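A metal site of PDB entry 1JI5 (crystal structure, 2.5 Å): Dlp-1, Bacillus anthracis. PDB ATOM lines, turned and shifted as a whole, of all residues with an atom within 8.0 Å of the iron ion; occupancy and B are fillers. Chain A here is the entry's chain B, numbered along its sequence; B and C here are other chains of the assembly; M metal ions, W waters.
The backbone carbonyl oxygen of His 36 of chain B lies within hydrogen-bond range of a ring nitrogen (ND1) of His 24 of chain B, at 2.7 Å. The side-chain carboxylate of Glu 55 lies within salt-bridge range of the side-chain amino group of Lys 132 of chain C, at 3.8 Å. The side-chain carboxylate of Asp 51 sits at hydrogen-bond distance from the indole nitrogen of Trp 25 of chain B (2.6 Å). The side-chain carboxylate (OE2) of Glu 55 lies close to a ring nitrogen (NE2) of His 36 of chain B, 3.5 Å away.
Three residues have an atom within 4 Å of the iron ion: Asp 51, Glu 55 and His 24 of chain B.
The side-chain carboxylate (OD2) of Asp 51 binds the iron ion, at 2.0 Å. The iron ion is bound by water W1 (2.0 Å). NE2 of His 24 of chain B binds the iron ion, at 2.1 Å. The iron ion is bound by OE2 of Glu 55, at 2.4 Å. The iron ion has four donor atoms within binding distance. Slightly farther from the iron ion lies OD1 of Asp 51 (2.7 Å).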
ATOM      1  N   ALA A  47      12.851  -1.635  11.782  1.00  0.00           N
ATOM      2  CA  ALA A  47      11.805  -1.642  12.800  1.00  0.00           C
ATOM      3  C   ALA A  47      12.398  -1.619  14.213  1.00  0.00           C
ATOM      4  O   ALA A  47      11.844  -0.990  15.123  1.00  0.00           O
ATOM      5  CB  ALA A  47      10.931  -2.848  12.622  1.00  0.00           C
ATOM      6  N   THR A  48      13.515  -2.310  14.394  1.00  0.00           N
ATOM      7  CA  THR A  48      14.162  -2.335  15.694  1.00  0.00           C
ATOM      8  C   THR A  48      14.557  -0.908  16.080  1.00  0.00           C
ATOM      9  O   THR A  48      14.249  -0.448  17.189  1.00  0.00           O
ATOM     10  CB  THR A  48      15.423  -3.208  15.705  1.00  0.00           C
ATOM     11  OG1 THR A  48      15.050  -4.566  15.448  1.00  0.00           O
ATOM     12  CG2 THR A  48      16.134  -3.129  17.058  1.00  0.00           C
ATOM     13  N   ILE A  50      13.442   1.987  15.010  1.00  0.00           N
ATOM     14  CA  ILE A  50      12.266   2.807  15.274  1.00  0.00           C
ATOM     15  C   ILE A  50      11.825   2.738  16.730  1.00  0.00           C
ATOM     16  O   ILE A  50      11.475   3.762  17.341  1.00  0.00           O
ATOM     17  CB  ILE A  50      11.051   2.380  14.390  1.00  0.00           C
ATOM     18  CG1 ILE A  50      11.367   2.597  12.900  1.00  0.00           C
ATOM     19  CG2 ILE A  50       9.803   3.156  14.795  1.00  0.00           C
ATOM     20  CD1 ILE A  50      10.261   2.055  11.970  1.00  0.00           C
ATOM     21  N   ASP A  51      11.824   1.545  17.311  1.00  0.00           N
ATOM     22  CA  ASP A  51      11.372   1.400  18.683  1.00  0.00           C
ATOM     23  C   ASP A  51      12.410   1.803  19.721  1.00  0.00           C
ATOM     24  O   ASP A  51      12.076   2.434  20.721  1.00  0.00           O
ATOM     25  CB  ASP A  51      10.904  -0.031  18.931  1.00  0.00           C
ATOM     26  CG  ASP A  51      10.026  -0.144  20.174  1.00  0.00           C
ATOM     27  OD1 ASP A  51       9.056   0.646  20.272  1.00  0.00           O
ATOM     28  OD2 ASP A  51      10.305  -1.000  21.032  1.00  0.00           O
ATOM     29  N   GLU A  52      13.669   1.440  19.487  1.00  0.00           N
ATOM     30  CA  GLU A  52      14.718   1.790  20.443  1.00  0.00           C
ATOM     31  C   GLU A  52      14.829   3.307  20.571  1.00  0.00           C
ATOM     32  O   GLU A  52      14.786   3.854  21.680  1.00  0.00           O
ATOM     33  CB  GLU A  52      16.056   1.257  19.973  1.00  0.00           C
ATOM     34  CG  GLU A  52      16.073  -0.188  19.565  1.00  0.00           C
ATOM     35  CD  GLU A  52      17.460  -0.616  19.122  1.00  0.00           C
ATOM     36  OE1 GLU A  52      18.028   0.079  18.257  1.00  0.00           O
ATOM     37  OE2 GLU A  52      17.974  -1.645  19.641  1.00  0.00           O
ATOM     38  N   ALA A  54      12.773   5.753  19.594  1.00  0.00           N
ATOM     39  CA  ALA A  54      11.553   6.312  20.180  1.00  0.00           C
ATOM     40  C   ALA A  54      11.574   6.153  21.700  1.00  0.00           C
ATOM     41  O   ALA A  54      11.385   7.114  22.449  1.00  0.00           O
ATOM     42  CB  ALA A  54      10.351   5.594  19.622  1.00  0.00           C
ATOM     43  N   GLU A  55      11.832   4.923  22.138  1.00  0.00           N
ATOM     44  CA  GLU A  55      11.878   4.640  23.565  1.00  0.00           C
ATOM     45  C   GLU A  55      13.082   5.337  24.204  1.00  0.00           C
ATOM     46  O   GLU A  55      13.134   5.497  25.429  1.00  0.00           O
ATOM     47  CB  GLU A  55      11.935   3.133  23.800  1.00  0.00           C
ATOM     48  CG  GLU A  55      10.783   2.374  23.152  1.00  0.00           C
ATOM     49  CD  GLU A  55      10.399   1.128  23.923  1.00  0.00           C
ATOM     50  OE1 GLU A  55      11.318   0.412  24.350  1.00  0.00           O
ATOM     51  OE2 GLU A  55       9.178   0.873  24.091  1.00  0.00           O
ATOM     52  N   LEU A  58      11.956   8.778  24.621  1.00  0.00           N
ATOM     53  CA  LEU A  58      10.906   8.584  25.595  1.00  0.00           C
ATOM     54  C   LEU A  58      11.543   8.495  26.990  1.00  0.00           C
ATOM     55  O   LEU A  58      10.964   8.918  27.974  1.00  0.00           O
ATOM     56  CB  LEU A  58      10.155   7.303  25.257  1.00  0.00           C
ATOM     57  CG  LEU A  58       8.678   7.187  25.572  1.00  0.00           C
ATOM     58  CD1 LEU A  58       7.929   8.415  25.118  1.00  0.00           C
ATOM     59  CD2 LEU A  58       8.149   5.968  24.866  1.00  0.00           C
ATOM     60  N   HIS B  21       2.252   1.747  17.442  1.00  0.00           N
ATOM     61  CA  HIS B  21       3.552   2.104  18.018  1.00  0.00           C
ATOM     62  C   HIS B  21       3.344   3.307  18.913  1.00  0.00           C
ATOM     63  O   HIS B  21       3.904   3.398  20.014  1.00  0.00           O
ATOM     64  CB  HIS B  21       4.543   2.493  16.924  1.00  0.00           C
ATOM     65  CG  HIS B  21       5.335   1.356  16.396  1.00  0.00           C
ATOM     66  ND1 HIS B  21       4.785   0.368  15.602  1.00  0.00           N
ATOM     67  CD2 HIS B  21       6.645   1.042  16.530  1.00  0.00           C
ATOM     68  CE1 HIS B  21       5.730  -0.497  15.263  1.00  0.00           C
ATOM     69  NE2 HIS B  21       6.865  -0.108  15.808  1.00  0.00           N
ATOM     70  N   HIS B  24       1.843   2.238  21.841  1.00  0.00           N
ATOM     71  CA  HIS B  24       2.878   1.460  22.505  1.00  0.00           C
ATOM     72  C   HIS B  24       3.741   2.441  23.299  1.00  0.00           C
ATOM     73  O   HIS B  24       4.036   2.208  24.458  1.00  0.00           O
ATOM     74  CB  HIS B  24       3.739   0.714  21.478  1.00  0.00           C
ATOM     75  CG  HIS B  24       4.927  -0.012  22.057  1.00  0.00           C
ATOM     76  ND1 HIS B  24       4.810  -1.078  22.927  1.00  0.00           N
ATOM     77  CD2 HIS B  24       6.269   0.155  21.857  1.00  0.00           C
ATOM     78  CE1 HIS B  24       6.022  -1.538  23.235  1.00  0.00           C
ATOM     79  NE2 HIS B  24       6.908  -0.808  22.595  1.00  0.00           N
ATOM     80  N   TRP B  25       4.110   3.544  22.659  1.00  0.00           N
ATOM     81  CA  TRP B  25       4.977   4.557  23.291  1.00  0.00           C
ATOM     82  C   TRP B  25       4.321   5.533  24.287  1.00  0.00           C
ATOM     83  O   TRP B  25       4.898   5.863  25.324  1.00  0.00           O
ATOM     84  CB  TRP B  25       5.684   5.374  22.199  1.00  0.00           C
ATOM     85  CG  TRP B  25       6.550   4.567  21.262  1.00  0.00           C
ATOM     86  CD1 TRP B  25       7.323   3.479  21.575  1.00  0.00           C
ATOM     87  CD2 TRP B  25       6.780   4.817  19.860  1.00  0.00           C
ATOM     88  NE1 TRP B  25       8.010   3.035  20.469  1.00  0.00           N
ATOM     89  CE2 TRP B  25       7.693   3.843  19.398  1.00  0.00           C
ATOM     90  CE3 TRP B  25       6.296   5.768  18.961  1.00  0.00           C
ATOM     91  CZ2 TRP B  25       8.141   3.791  18.076  1.00  0.00           C
ATOM     92  CZ3 TRP B  25       6.736   5.723  17.639  1.00  0.00           C
ATOM     93  CH2 TRP B  25       7.647   4.729  17.213  1.00  0.00           C
ATOM     94  N   HIS B  36       1.364  -1.780  27.279  1.00  0.00           N
ATOM     95  CA  HIS B  36       2.581  -1.462  26.533  1.00  0.00           C
ATOM     96  C   HIS B  36       2.896  -2.709  25.736  1.00  0.00           C
ATOM     97  O   HIS B  36       3.256  -2.647  24.552  1.00  0.00           O
ATOM     98  CB  HIS B  36       3.724  -1.162  27.517  1.00  0.00           C
ATOM     99  CG  HIS B  36       5.065  -0.955  26.873  1.00  0.00           C
ATOM    100  ND1 HIS B  36       5.352   0.134  26.087  1.00  0.00           N
ATOM    101  CD2 HIS B  36       6.206  -1.670  26.953  1.00  0.00           C
ATOM    102  CE1 HIS B  36       6.621   0.084  25.704  1.00  0.00           C
ATOM    103  NE2 HIS B  36       7.163  -1.002  26.221  1.00  0.00           N
ATOM    104  N   GLU B  37       2.739  -3.840  26.398  1.00  0.00           N
ATOM    105  CA  GLU B  37       3.006  -5.141  25.821  1.00  0.00           C
ATOM    106  C   GLU B  37       1.996  -5.496  24.731  1.00  0.00           C
ATOM    107  O   GLU B  37       2.372  -5.768  23.585  1.00  0.00           O
ATOM    108  CB  GLU B  37       2.985  -6.186  26.930  1.00  0.00           C
ATOM    109  CG  GLU B  37       3.429  -7.564  26.512  1.00  0.00           C
ATOM    110  CD  GLU B  37       3.634  -8.497  27.696  1.00  0.00           C
ATOM    111  OE1 GLU B  37       4.417  -8.144  28.607  1.00  0.00           O
ATOM    112  OE2 GLU B  37       3.017  -9.599  27.706  1.00  0.00           O
ATOM    113  N   GLU B  40       2.436  -3.895  21.330  1.00  0.00           N
ATOM    114  CA  GLU B  40       3.563  -4.404  20.563  1.00  0.00           C
ATOM    115  C   GLU B  40       3.187  -5.726  19.871  1.00  0.00           C
ATOM    116  O   GLU B  40       3.616  -6.016  18.742  1.00  0.00           O
ATOM    117  CB  GLU B  40       4.784  -4.608  21.477  1.00  0.00           C
ATOM    118  CG  GLU B  40       5.921  -5.377  20.839  1.00  0.00           C
ATOM    119  CD  GLU B  40       7.243  -5.124  21.525  1.00  0.00           C
ATOM    120  OE1 GLU B  40       7.249  -4.956  22.764  1.00  0.00           O
ATOM    121  OE2 GLU B  40       8.292  -5.100  20.829  1.00  0.00           O
ATOM    122  N   TYR B  43       1.027  -4.617  16.858  1.00  0.00           N
ATOM    123  CA  TYR B  43       1.691  -4.069  15.693  1.00  0.00           C
ATOM    124  C   TYR B  43       2.588  -5.086  15.048  1.00  0.00           C
ATOM    125  O   TYR B  43       2.921  -4.966  13.867  1.00  0.00           O
ATOM    126  CB  TYR B  43       2.453  -2.759  15.989  1.00  0.00           C
ATOM    127  CG  TYR B  43       3.665  -2.785  16.908  1.00  0.00           C
ATOM    128  CD1 TYR B  43       4.804  -3.524  16.598  1.00  0.00           C
ATOM    129  CD2 TYR B  43       3.688  -1.970  18.053  1.00  0.00           C
ATOM    130  CE1 TYR B  43       5.959  -3.455  17.406  1.00  0.00           C
ATOM    131  CE2 TYR B  43       4.830  -1.884  18.852  1.00  0.00           C
ATOM    132  CZ  TYR B  43       5.959  -2.633  18.525  1.00  0.00           C
ATOM    133  OH  TYR B  43       7.083  -2.536  19.313  1.00  0.00           O
ATOM    134  N   LYS C 132      15.563   3.875  31.120  1.00  0.00           N
ATOM    135  CA  LYS C 132      14.404   3.266  30.491  1.00  0.00           C
ATOM    136  C   LYS C 132      13.428   2.862  31.584  1.00  0.00           C
ATOM    137  O   LYS C 132      12.237   3.192  31.530  1.00  0.00           O
ATOM    138  CB  LYS C 132      14.846   2.051  29.684  1.00  0.00           C
ATOM    139  CG  LYS C 132      13.810   1.514  28.708  1.00  0.00           C
ATOM    140  CD  LYS C 132      14.379   0.295  27.975  1.00  0.00           C
ATOM    141  CE  LYS C 132      13.404  -0.275  26.948  1.00  0.00           C
ATOM    142  NZ  LYS C 132      13.939  -1.506  26.267  1.00  0.00           N
ATOM    143  N   TRP C 135      11.484   5.657  33.126  1.00  0.00           N
ATOM    144  CA  TRP C 135      10.407   6.092  32.254  1.00  0.00           C
ATOM    145  C   TRP C 135       9.172   5.203  32.412  1.00  0.00           C
ATOM    146  O   TRP C 135       8.049   5.695  32.617  1.00  0.00           O
ATOM    147  CB  TRP C 135      10.884   6.113  30.790  1.00  0.00           C
ATOM    148  CG  TRP C 135       9.794   5.767  29.792  1.00  0.00           C
ATOM    149  CD1 TRP C 135       8.533   6.314  29.731  1.00  0.00           C
ATOM    150  CD2 TRP C 135       9.798   4.705  28.829  1.00  0.00           C
ATOM    151  NE1 TRP C 135       7.765   5.660  28.804  1.00  0.00           N
ATOM    152  CE2 TRP C 135       8.513   4.655  28.235  1.00  0.00           C
ATOM    153  CE3 TRP C 135      10.769   3.772  28.408  1.00  0.00           C
ATOM    154  CZ2 TRP C 135       8.166   3.722  27.239  1.00  0.00           C
ATOM    155  CZ3 TRP C 135      10.419   2.836  27.421  1.00  0.00           C
ATOM    156  CH2 TRP C 135       9.127   2.819  26.859  1.00  0.00           C
ATOM    157  N   MET C 136       9.376   3.895  32.307  1.00  0.00           N
ATOM    158  CA  MET C 136       8.287   2.944  32.425  1.00  0.00           C
ATOM    159  C   MET C 136       7.682   2.998  33.828  1.00  0.00           C
ATOM    160  O   MET C 136       6.451   2.993  33.984  1.00  0.00           O
ATOM    161  CB  MET C 136       8.790   1.531  32.119  1.00  0.00           C
ATOM    162  CG  MET C 136       9.455   1.391  30.756  1.00  0.00           C
ATOM    163  SD  MET C 136       9.765  -0.352  30.295  1.00  0.00           S
ATOM    164  CE  MET C 136      10.471  -1.002  31.858  1.00  0.00           C
HETATM  165 FE    FE M   1       8.954  -0.916  22.486  1.00  0.00          FE
HETATM  166  O   HOH W   1       8.990  -2.797  23.292  1.00  0.00           O
